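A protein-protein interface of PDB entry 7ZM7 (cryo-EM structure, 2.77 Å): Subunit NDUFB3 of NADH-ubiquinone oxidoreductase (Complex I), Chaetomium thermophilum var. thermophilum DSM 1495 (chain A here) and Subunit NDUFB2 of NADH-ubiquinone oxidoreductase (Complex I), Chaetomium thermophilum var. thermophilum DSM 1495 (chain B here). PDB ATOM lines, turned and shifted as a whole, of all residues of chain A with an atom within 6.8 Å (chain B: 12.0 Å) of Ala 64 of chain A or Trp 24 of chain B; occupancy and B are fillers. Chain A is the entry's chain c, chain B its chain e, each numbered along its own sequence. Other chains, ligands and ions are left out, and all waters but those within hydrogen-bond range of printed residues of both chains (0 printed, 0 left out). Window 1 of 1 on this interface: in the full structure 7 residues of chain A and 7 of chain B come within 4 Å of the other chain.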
ATOM      1  N   LEU A  58      -3.532 -24.454  19.064  1.00  0.00           N
ATOM      2  CA  LEU A  58      -3.826 -24.237  17.648  1.00  0.00           C
ATOM      3  C   LEU A  58      -4.913 -25.220  17.250  1.00  0.00           C
ATOM      4  O   LEU A  58      -4.605 -26.335  16.792  1.00  0.00           O
ATOM      5  CB  LEU A  58      -2.580 -24.429  16.787  1.00  0.00           C
ATOM      6  CG  LEU A  58      -1.593 -23.265  16.641  1.00  0.00           C
ATOM      7  CD1 LEU A  58      -2.258 -22.088  15.952  1.00  0.00           C
ATOM      8  CD2 LEU A  58      -0.975 -22.840  17.963  1.00  0.00           C
ATOM      9  N   PRO A  59      -6.185 -24.865  17.406  1.00  0.00           N
ATOM     10  CA  PRO A  59      -7.257 -25.864  17.303  1.00  0.00           C
ATOM     11  C   PRO A  59      -7.322 -26.585  15.968  1.00  0.00           C
ATOM     12  O   PRO A  59      -7.211 -27.814  15.919  1.00  0.00           O
ATOM     13  CB  PRO A  59      -8.526 -25.036  17.543  1.00  0.00           C
ATOM     14  CG  PRO A  59      -8.132 -23.630  17.248  1.00  0.00           C
ATOM     15  CD  PRO A  59      -6.707 -23.516  17.667  1.00  0.00           C
ATOM     16  N   GLY A  60      -7.494 -25.843  14.881  1.00  0.00           N
ATOM     17  CA  GLY A  60      -7.691 -26.433  13.575  1.00  0.00           C
ATOM     18  C   GLY A  60      -6.433 -26.714  12.787  1.00  0.00           C
ATOM     19  O   GLY A  60      -6.529 -27.200  11.655  1.00  0.00           O
ATOM     20  N   PHE A  61      -5.255 -26.445  13.349  1.00  0.00           N
ATOM     21  CA  PHE A  61      -4.026 -26.547  12.572  1.00  0.00           C
ATOM     22  C   PHE A  61      -3.797 -27.967  12.078  1.00  0.00           C
ATOM     23  O   PHE A  61      -3.414 -28.174  10.922  1.00  0.00           O
ATOM     24  CB  PHE A  61      -2.839 -26.075  13.409  1.00  0.00           C
ATOM     25  CG  PHE A  61      -1.709 -25.530  12.595  1.00  0.00           C
ATOM     26  CD1 PHE A  61      -1.760 -24.244  12.093  1.00  0.00           C
ATOM     27  CD2 PHE A  61      -0.596 -26.304  12.328  1.00  0.00           C
ATOM     28  CE1 PHE A  61      -0.722 -23.739  11.341  1.00  0.00           C
ATOM     29  CE2 PHE A  61       0.444 -25.805  11.577  1.00  0.00           C
ATOM     30  CZ  PHE A  61       0.383 -24.522  11.085  1.00  0.00           C
ATOM     31  N   GLY A  62      -4.028 -28.959  12.937  1.00  0.00           N
ATOM     32  CA  GLY A  62      -3.818 -30.335  12.526  1.00  0.00           C
ATOM     33  C   GLY A  62      -4.759 -30.765  11.419  1.00  0.00           C
ATOM     34  O   GLY A  62      -4.335 -31.375  10.434  1.00  0.00           O
ATOM     35  N   ILE A  63      -6.043 -30.454  11.562  1.00  0.00           N
ATOM     36  CA  ILE A  63      -7.020 -30.845  10.553  1.00  0.00           C
ATOM     37  C   ILE A  63      -6.754 -30.118   9.241  1.00  0.00           C
ATOM     38  O   ILE A  63      -6.854 -30.706   8.158  1.00  0.00           O
ATOM     39  CB  ILE A  63      -8.448 -30.588  11.065  1.00  0.00           C
ATOM     40  CG1 ILE A  63      -8.741 -31.447  12.297  1.00  0.00           C
ATOM     41  CG2 ILE A  63      -9.462 -30.874   9.975  1.00  0.00           C
ATOM     42  CD1 ILE A  63      -8.363 -30.806  13.623  1.00  0.00           C
ATOM     43  N   ALA A  64      -6.408 -28.833   9.316  1.00  0.00           N
ATOM     44  CA  ALA A  64      -6.192 -28.058   8.101  1.00  0.00           C
ATOM     45  C   ALA A  64      -4.946 -28.516   7.354  1.00  0.00           C
ATOM     46  O   ALA A  64      -4.957 -28.611   6.122  1.00  0.00           O
ATOM     47  CB  ALA A  64      -6.093 -26.574   8.441  1.00  0.00           C
ATOM     48  N   THR A  65      -3.865 -28.805   8.080  1.00  0.00           N
ATOM     49  CA  THR A  65      -2.589 -29.087   7.429  1.00  0.00           C
ATOM     50  C   THR A  65      -2.678 -30.327   6.552  1.00  0.00           C
ATOM     51  O   THR A  65      -2.208 -30.329   5.409  1.00  0.00           O
ATOM     52  CB  THR A  65      -1.488 -29.245   8.475  1.00  0.00           C
ATOM     53  OG1 THR A  65      -1.371 -28.035   9.232  1.00  0.00           O
ATOM     54  CG2 THR A  65      -0.159 -29.536   7.804  1.00  0.00           C
ATOM     55  N   VAL A  66      -3.287 -31.396   7.067  1.00  0.00           N
ATOM     56  CA  VAL A  66      -3.466 -32.592   6.252  1.00  0.00           C
ATOM     57  C   VAL A  66      -4.452 -32.319   5.123  1.00  0.00           C
ATOM     58  O   VAL A  66      -4.276 -32.802   3.998  1.00  0.00           O
ATOM     59  CB  VAL A  66      -3.905 -33.781   7.126  1.00  0.00           C
ATOM     60  CG1 VAL A  66      -5.148 -33.434   7.921  1.00  0.00           C
ATOM     61  CG2 VAL A  66      -4.149 -35.009   6.266  1.00  0.00           C
ATOM     62  N   ALA A  67      -5.493 -31.532   5.399  1.00  0.00           N
ATOM     63  CA  ALA A  67      -6.462 -31.204   4.361  1.00  0.00           C
ATOM     64  C   ALA A  67      -5.825 -30.385   3.247  1.00  0.00           C
ATOM     65  O   ALA A  67      -6.095 -30.615   2.063  1.00  0.00           O
ATOM     66  CB  ALA A  67      -7.647 -30.454   4.968  1.00  0.00           C
ATOM     67  N   PHE A  68      -4.974 -29.421   3.605  1.00  0.00           N
ATOM     68  CA  PHE A  68      -4.324 -28.605   2.586  1.00  0.00           C
ATOM     69  C   PHE A  68      -3.386 -29.429   1.718  1.00  0.00           C
ATOM     70  O   PHE A  68      -3.313 -29.203   0.505  1.00  0.00           O
ATOM     71  CB  PHE A  68      -3.557 -27.455   3.232  1.00  0.00           C
ATOM     72  CG  PHE A  68      -2.903 -26.540   2.242  1.00  0.00           C
ATOM     73  CD1 PHE A  68      -3.649 -25.607   1.547  1.00  0.00           C
ATOM     74  CD2 PHE A  68      -1.545 -26.621   1.999  1.00  0.00           C
ATOM     75  CE1 PHE A  68      -3.052 -24.768   0.634  1.00  0.00           C
ATOM     76  CE2 PHE A  68      -0.943 -25.784   1.087  1.00  0.00           C
ATOM     77  CZ  PHE A  68      -1.697 -24.857   0.402  1.00  0.00           C
ATOM     78  N   THR A  69      -2.661 -30.377   2.313  1.00  0.00           N
ATOM     79  CA  THR A  69      -1.779 -31.229   1.522  1.00  0.00           C
ATOM     80  C   THR A  69      -2.571 -32.039   0.506  1.00  0.00           C
ATOM     81  O   THR A  69      -2.064 -32.365  -0.572  1.00  0.00           O
ATOM     82  CB  THR A  69      -0.976 -32.151   2.435  1.00  0.00           C
ATOM     83  OG1 THR A  69      -1.868 -32.841   3.317  1.00  0.00           O
ATOM     84  CG2 THR A  69       0.019 -31.347   3.251  1.00  0.00           C
ATOM     85  N   ALA A  70      -3.819 -32.375   0.835  1.00  0.00           N
ATOM     86  CA  ALA A  70      -4.684 -33.017  -0.146  1.00  0.00           C
ATOM     87  C   ALA A  70      -4.956 -32.085  -1.319  1.00  0.00           C
ATOM     88  O   ALA A  70      -4.990 -32.520  -2.475  1.00  0.00           O
ATOM     89  CB  ALA A  70      -5.991 -33.458   0.510  1.00  0.00           C
ATOM     90  N   PHE B  14     -17.121 -28.711  18.261  1.00  0.00           N
ATOM     91  CA  PHE B  14     -17.081 -28.826  16.783  1.00  0.00           C
ATOM     92  C   PHE B  14     -16.948 -27.427  16.190  1.00  0.00           C
ATOM     93  O   PHE B  14     -16.117 -27.236  15.287  1.00  0.00           O
ATOM     94  CB  PHE B  14     -18.336 -29.517  16.253  1.00  0.00           C
ATOM     95  CG  PHE B  14     -18.489 -29.470  14.754  1.00  0.00           C
ATOM     96  CD1 PHE B  14     -17.657 -30.211  13.932  1.00  0.00           C
ATOM     97  CD2 PHE B  14     -19.468 -28.687  14.166  1.00  0.00           C
ATOM     98  CE1 PHE B  14     -17.797 -30.166  12.555  1.00  0.00           C
ATOM     99  CE2 PHE B  14     -19.609 -28.643  12.788  1.00  0.00           C
ATOM    100  CZ  PHE B  14     -18.774 -29.383  11.985  1.00  0.00           C
ATOM    101  N   LEU B  15     -17.718 -26.470  16.712  1.00  0.00           N
ATOM    102  CA  LEU B  15     -17.679 -25.116  16.112  1.00  0.00           C
ATOM    103  C   LEU B  15     -16.273 -24.556  16.291  1.00  0.00           C
ATOM    104  O   LEU B  15     -15.739 -24.020  15.316  1.00  0.00           O
ATOM    105  CB  LEU B  15     -18.708 -24.214  16.796  1.00  0.00           C
ATOM    106  CG  LEU B  15     -20.075 -24.153  16.122  1.00  0.00           C
ATOM    107  CD1 LEU B  15     -20.972 -23.142  16.819  1.00  0.00           C
ATOM    108  CD2 LEU B  15     -19.928 -23.805  14.650  1.00  0.00           C
ATOM    109  N   ALA B  16     -15.688 -24.725  17.476  1.00  0.00           N
ATOM    110  CA  ALA B  16     -14.360 -24.122  17.741  1.00  0.00           C
ATOM    111  C   ALA B  16     -13.291 -24.722  16.824  1.00  0.00           C
ATOM    112  O   ALA B  16     -12.481 -23.954  16.289  1.00  0.00           O
ATOM    113  CB  ALA B  16     -13.997 -24.292  19.192  1.00  0.00           C
ATOM    114  N   THR B  17     -13.295 -26.045  16.655  1.00  0.00           N
ATOM    115  CA  THR B  17     -12.291 -26.705  15.780  1.00  0.00           C
ATOM    116  C   THR B  17     -12.511 -26.264  14.331  1.00  0.00           C
ATOM    117  O   THR B  17     -11.518 -26.019  13.632  1.00  0.00           O
ATOM    118  CB  THR B  17     -12.313 -28.226  15.958  1.00  0.00           C
ATOM    119  OG1 THR B  17     -12.193 -28.493  17.355  1.00  0.00           O
ATOM    120  CG2 THR B  17     -11.204 -28.925  15.205  1.00  0.00           C
ATOM    121  N   GLY B  18     -13.770 -26.175  13.905  1.00  0.00           N
ATOM    122  CA  GLY B  18     -14.080 -25.780  12.519  1.00  0.00           C
ATOM    123  C   GLY B  18     -13.633 -24.361  12.257  1.00  0.00           C
ATOM    124  O   GLY B  18     -13.092 -24.104  11.178  1.00  0.00           O
ATOM    125  N   LEU B  19     -13.902 -23.453  13.191  1.00  0.00           N
ATOM    126  CA  LEU B  19     -13.384 -22.100  13.043  1.00  0.00           C
ATOM    127  C   LEU B  19     -11.865 -22.093  13.015  1.00  0.00           C
ATOM    128  O   LEU B  19     -11.260 -21.212  12.396  1.00  0.00           O
ATOM    129  CB  LEU B  19     -13.908 -21.218  14.167  1.00  0.00           C
ATOM    130  CG  LEU B  19     -15.405 -20.967  14.059  1.00  0.00           C
ATOM    131  CD1 LEU B  19     -15.936 -20.326  15.330  1.00  0.00           C
ATOM    132  CD2 LEU B  19     -15.692 -20.103  12.853  1.00  0.00           C
ATOM    133  N   GLY B  20     -11.235 -23.055  13.685  1.00  0.00           N
ATOM    134  CA  GLY B  20      -9.813 -23.259  13.486  1.00  0.00           C
ATOM    135  C   GLY B  20      -9.496 -23.683  12.068  1.00  0.00           C
ATOM    136  O   GLY B  20      -8.525 -23.215  11.471  1.00  0.00           O
ATOM    137  N   ALA B  21     -10.316 -24.570  11.506  1.00  0.00           N
ATOM    138  CA  ALA B  21     -10.149 -24.943  10.109  1.00  0.00           C
ATOM    139  C   ALA B  21     -10.435 -23.781   9.170  1.00  0.00           C
ATOM    140  O   ALA B  21     -10.027 -23.828   8.007  1.00  0.00           O
ATOM    141  CB  ALA B  21     -11.054 -26.125   9.765  1.00  0.00           C
ATOM    142  N   SER B  22     -11.136 -22.748   9.639  1.00  0.00           N
ATOM    143  CA  SER B  22     -11.314 -21.556   8.820  1.00  0.00           C
ATOM    144  C   SER B  22      -9.976 -20.874   8.567  1.00  0.00           C
ATOM    145  O   SER B  22      -9.635 -20.560   7.422  1.00  0.00           O
ATOM    146  CB  SER B  22     -12.299 -20.600   9.490  1.00  0.00           C
ATOM    147  OG  SER B  22     -13.625 -21.087   9.384  1.00  0.00           O
ATOM    148  N   MET B  23      -9.192 -20.656   9.620  1.00  0.00           N
ATOM    149  CA  MET B  23      -7.793 -20.323   9.420  1.00  0.00           C
ATOM    150  C   MET B  23      -7.056 -21.519   8.844  1.00  0.00           C
ATOM    151  O   MET B  23      -7.612 -22.605   8.661  1.00  0.00           O
ATOM    152  CB  MET B  23      -7.096 -19.946  10.718  1.00  0.00           C
ATOM    153  CG  MET B  23      -7.800 -19.110  11.726  1.00  0.00           C
ATOM    154  SD  MET B  23      -6.411 -18.617  12.770  1.00  0.00           S
ATOM    155  CE  MET B  23      -7.099 -17.333  13.771  1.00  0.00           C
ATOM    156  N   TRP B  24      -5.774 -21.306   8.555  1.00  0.00           N
ATOM    157  CA  TRP B  24      -4.842 -22.387   8.268  1.00  0.00           C
ATOM    158  C   TRP B  24      -5.289 -23.184   7.054  1.00  0.00           C
ATOM    159  O   TRP B  24      -4.697 -24.210   6.712  1.00  0.00           O
ATOM    160  CB  TRP B  24      -4.698 -23.302   9.481  1.00  0.00           C
ATOM    161  CG  TRP B  24      -4.632 -22.576  10.781  1.00  0.00           C
ATOM    162  CD1 TRP B  24      -5.447 -22.755  11.846  1.00  0.00           C
ATOM    163  CD2 TRP B  24      -3.691 -21.570  11.158  1.00  0.00           C
ATOM    164  NE1 TRP B  24      -5.080 -21.920  12.865  1.00  0.00           N
ATOM    165  CE2 TRP B  24      -4.000 -21.183  12.466  1.00  0.00           C
ATOM    166  CE3 TRP B  24      -2.612 -20.963  10.515  1.00  0.00           C
ATOM    167  CZ2 TRP B  24      -3.277 -20.214  13.144  1.00  0.00           C
ATOM    168  CZ3 TRP B  24      -1.898 -20.010  11.183  1.00  0.00           C
ATOM    169  CH2 TRP B  24      -2.230 -19.639  12.485  1.00  0.00           C
ATOM    170  N   PHE B  25      -6.350 -22.773   6.461  1.00  0.00           N
ATOM    171  CA  PHE B  25      -6.709 -23.219   5.135  1.00  0.00           C
ATOM    172  C   PHE B  25      -6.962 -22.027   4.248  1.00  0.00           C
ATOM    173  O   PHE B  25      -6.687 -22.086   3.049  1.00  0.00           O
ATOM    174  CB  PHE B  25      -7.933 -24.125   5.151  1.00  0.00           C
ATOM    175  CG  PHE B  25      -8.226 -24.752   3.827  1.00  0.00           C
ATOM    176  CD1 PHE B  25      -7.583 -25.913   3.444  1.00  0.00           C
ATOM    177  CD2 PHE B  25      -9.131 -24.177   2.960  1.00  0.00           C
ATOM    178  CE1 PHE B  25      -7.845 -26.490   2.224  1.00  0.00           C
ATOM    179  CE2 PHE B  25      -9.397 -24.751   1.739  1.00  0.00           C
ATOM    180  CZ  PHE B  25      -8.754 -25.908   1.371  1.00  0.00           C
ATOM    181  N   TRP B  26      -7.495 -20.948   4.816  1.00  0.00           N
ATOM    182  CA  TRP B  26      -7.440 -19.660   4.154  1.00  0.00           C
ATOM    183  C   TRP B  26      -6.010 -19.151   4.121  1.00  0.00           C
ATOM    184  O   TRP B  26      -5.599 -18.483   3.167  1.00  0.00           O
ATOM    185  CB  TRP B  26      -8.356 -18.677   4.874  1.00  0.00           C
ATOM    186  CG  TRP B  26      -8.487 -17.374   4.191  1.00  0.00           C
ATOM    187  CD1 TRP B  26      -8.048 -16.170   4.633  1.00  0.00           C
ATOM    188  CD2 TRP B  26      -9.112 -17.138   2.930  1.00  0.00           C
ATOM    189  NE1 TRP B  26      -8.357 -15.192   3.724  1.00  0.00           N
ATOM    190  CE2 TRP B  26      -9.011 -15.764   2.668  1.00  0.00           C
ATOM    191  CE3 TRP B  26      -9.744 -17.957   1.997  1.00  0.00           C
ATOM    192  CZ2 TRP B  26      -9.517 -15.189   1.512  1.00  0.00           C
ATOM    193  CZ3 TRP B  26     -10.247 -17.386   0.850  1.00  0.00           C
ATOM    194  CH2 TRP B  26     -10.130 -16.015   0.616  1.00  0.00           C
ATOM    195  N   ILE B  27      -5.239 -19.473   5.159  1.00  0.00           N
ATOM    196  CA  ILE B  27      -3.865 -18.998   5.264  1.00  0.00           C
ATOM    197  C   ILE B  27      -3.010 -19.556   4.142  1.00  0.00           C
ATOM    198  O   ILE B  27      -2.459 -18.807   3.329  1.00  0.00           O
ATOM    199  CB  ILE B  27      -3.284 -19.357   6.639  1.00  0.00           C
ATOM    200  CG1 ILE B  27      -4.117 -18.716   7.724  1.00  0.00           C
ATOM    201  CG2 ILE B  27      -1.840 -18.918   6.744  1.00  0.00           C
ATOM    202  CD1 ILE B  27      -4.098 -17.254   7.604  1.00  0.00           C
ATOM    203  N   PHE B  28      -2.886 -20.873   4.076  1.00  0.00           N
ATOM    204  CA  PHE B  28      -2.037 -21.450   3.046  1.00  0.00           C
ATOM    205  C   PHE B  28      -2.614 -21.222   1.659  1.00  0.00           C
ATOM    206  O   PHE B  28      -1.862 -21.024   0.702  1.00  0.00           O
ATOM    207  CB  PHE B  28      -1.803 -22.930   3.322  1.00  0.00           C
ATOM    208  CG  PHE B  28      -1.290 -23.207   4.701  1.00  0.00           C
ATOM    209  CD1 PHE B  28      -2.148 -23.324   5.770  1.00  0.00           C
ATOM    210  CD2 PHE B  28       0.068 -23.352   4.920  1.00  0.00           C
ATOM    211  CE1 PHE B  28      -1.672 -23.580   7.028  1.00  0.00           C
ATOM    212  CE2 PHE B  28       0.552 -23.607   6.181  1.00  0.00           C
ATOM    213  CZ  PHE B  28      -0.324 -23.721   7.238  1.00  0.00           C
ATOM    214  N   TYR B  29      -3.936 -21.214   1.524  1.00  0.00           N
ATOM    215  CA  TYR B  29      -4.501 -20.964   0.207  1.00  0.00           C
ATOM    216  C   TYR B  29      -4.150 -19.570  -0.278  1.00  0.00           C
ATOM    217  O   TYR B  29      -3.885 -19.367  -1.467  1.00  0.00           O
ATOM    218  CB  TYR B  29      -6.010 -21.150   0.208  1.00  0.00           C
ATOM    219  CG  TYR B  29      -6.588 -21.003  -1.172  1.00  0.00           C
ATOM    220  CD1 TYR B  29      -6.382 -21.980  -2.131  1.00  0.00           C
ATOM    221  CD2 TYR B  29      -7.309 -19.878  -1.527  1.00  0.00           C
ATOM    222  CE1 TYR B  29      -6.898 -21.851  -3.397  1.00  0.00           C
ATOM    223  CE2 TYR B  29      -7.828 -19.739  -2.792  1.00  0.00           C
ATOM    224  CZ  TYR B  29      -7.618 -20.729  -3.724  1.00  0.00           C
ATOM    225  OH  TYR B  29      -8.134 -20.597  -4.991  1.00  0.00           O
ATOM    226  N   ARG B  30      -4.161 -18.591   0.622  1.00  0.00           N
ATOM    227  CA  ARG B  30      -3.744 -17.252   0.234  1.00  0.00           C
ATOM    228  C   ARG B  30      -2.229 -17.163   0.126  1.00  0.00           C
ATOM    229  O   ARG B  30      -1.701 -16.497  -0.772  1.00  0.00           O
ATOM    230  CB  ARG B  30      -4.289 -16.230   1.224  1.00  0.00           C
ATOM    231  CG  ARG B  30      -5.764 -15.946   1.033  1.00  0.00           C
ATOM    232  CD  ARG B  30      -5.965 -14.645   0.302  1.00  0.00           C
ATOM    233  NE  ARG B  30      -5.559 -14.723  -1.094  1.00  0.00           N
ATOM    234  CZ  ARG B  30      -6.314 -15.229  -2.062  1.00  0.00           C
ATOM    235  NH1 ARG B  30      -7.521 -15.698  -1.784  1.00  0.00           N
ATOM    236  NH2 ARG B  30      -5.867 -15.256  -3.308  1.00  0.00           N
ATOM    237  N   ALA B  31      -1.515 -17.840   1.023  1.00  0.00           N
ATOM    238  CA  ALA B  31      -0.061 -17.875   0.931  1.00  0.00           C
ATOM    239  C   ALA B  31       0.394 -18.606  -0.321  1.00  0.00           C
ATOM    240  O   ALA B  31       1.364 -18.198  -0.966  1.00  0.00           O
ATOM    241  CB  ALA B  31       0.531 -18.528   2.178  1.00  0.00           C
ATOM    242  N   LYS B  32      -0.283 -19.692  -0.683  1.00  0.00           N
ATOM    243  CA  LYS B  32       0.108 -20.403  -1.893  1.00  0.00           C
ATOM    244  C   LYS B  32      -0.187 -19.582  -3.142  1.00  0.00           C
ATOM    245  O   LYS B  32       0.584 -19.627  -4.107  1.00  0.00           O
ATOM    246  CB  LYS B  32      -0.594 -21.757  -1.966  1.00  0.00           C
ATOM    247  CG  LYS B  32      -0.438 -22.457  -3.306  1.00  0.00           C
ATOM    248  CD  LYS B  32      -0.875 -23.907  -3.238  1.00  0.00           C
ATOM    249  CE  LYS B  32      -1.023 -24.494  -4.627  1.00  0.00           C
ATOM    250  NZ  LYS B  32      -2.061 -23.775  -5.415  1.00  0.00           N
ATOM    251  N   LYS B  33      -1.276 -18.817  -3.142  1.00  0.00           N
ATOM    252  CA  LYS B  33      -1.703 -18.116  -4.346  1.00  0.00           C
ATOM    253  C   LYS B  33      -1.122 -16.713  -4.456  1.00  0.00           C
ATOM    254  O   LYS B  33      -0.738 -16.291  -5.551  1.00  0.00           O
ATOM    255  CB  LYS B  33      -3.231 -18.055  -4.395  1.00  0.00           C
ATOM    256  CG  LYS B  33      -3.790 -17.422  -5.650  1.00  0.00           C
ATOM    257  CD  LYS B  33      -5.309 -17.454  -5.638  1.00  0.00           C
ATOM    258  CE  LYS B  33      -5.888 -16.906  -6.929  1.00  0.00           C
ATOM    259  NZ  LYS B  33      -5.629 -15.447  -7.071  1.00  0.00           N
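The side-chain sulfur of Met 23 of chain B sits close to the indole nitrogen of Trp 24 of chain B.
The side-chain hydroxyl (OG1) of Thr 65 of chain A lies within hydrogen-bond range of the backbone carbonyl oxygen (O) of Phe 61 of chain A.
Leu 58 of chain A touches just one residue of chain B: Trp 24.
Gly 62 of chain A touches none of the printed residues of chain B.
No residue of chain B comes within 4 Å of Val 66 of chain A.
No residue of chain B comes within 4 Å of Ala 67 of chain A.
Of the printed residues of chain B, Phe 68 of chain A touches Phe 28 (3.5 Å), Tyr 29 (3.8 Å) and Lys 32 (3.9 Å).
Of the printed residues of chain A, Gly 20 of chain B touches Gly 60 (3.6 Å).
Of the printed residues of chain B, Phe 61 of chain A touches Trp 24 (3.4 Å) and Phe 28 (3.99 Å).
Printed residues of chain A within 4 Å of Ala 21 of chain B: Gly 60.
Of the printed residues of chain A, Phe 28 of chain B touches Phe 61 and Phe 68.
Printed residues of chain A within 4 Å of Lys 32 of chain B: Phe 68 (3.9 Å).
The nearest residue of chain B that does not touch Ala 64 of chain A is Met 23 of chain B (4.3 Å).
The nearest printed residue of chain B that does not touch Phe 61 of chain A is Gly 20 of chain B (5.0 Å).
Leu 58 of chain A touches Trp 24 of chain B (CD1 to CZ2, 3.5 Å).
Thr 17 of chain B touches Gly 60 of chain A.
CA of Gly 60 of chain A touches C of Gly 20 of chain B (3.6 Å).
Ala 21 of chain B touches Gly 60 of chain A.
Phe 61 of chain A touches Phe 28 of chain B (CZ to CZ, 3.99 Å).
Thr 17 of chain B touches Ile 63 of chain A.
Ala 64 of chain A touches Trp 24 of chain B.
CE1 of Phe 68 of chain A touches CB of Phe 28 of chain B (3.5 Å).
CE1 of Phe 68 of chain A touches N of Tyr 29 of chain B, at 3.8 Å.
Phe 68 of chain A touches Lys 32 of chain B.
Of the 20 printed residues of chain B, 7 touch a printed residue of chain A.
Hydrophobic or aromatic side chains of chain A within 4 Å of the printed part of chain B: Leu 58, Phe 61, Ile 63, Ala 64 and Phe 68.
Among the printed residues, no Asp or Glu carboxylate lies within 4 Å of a Lys or Arg side-chain nitrogen of the other chain.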
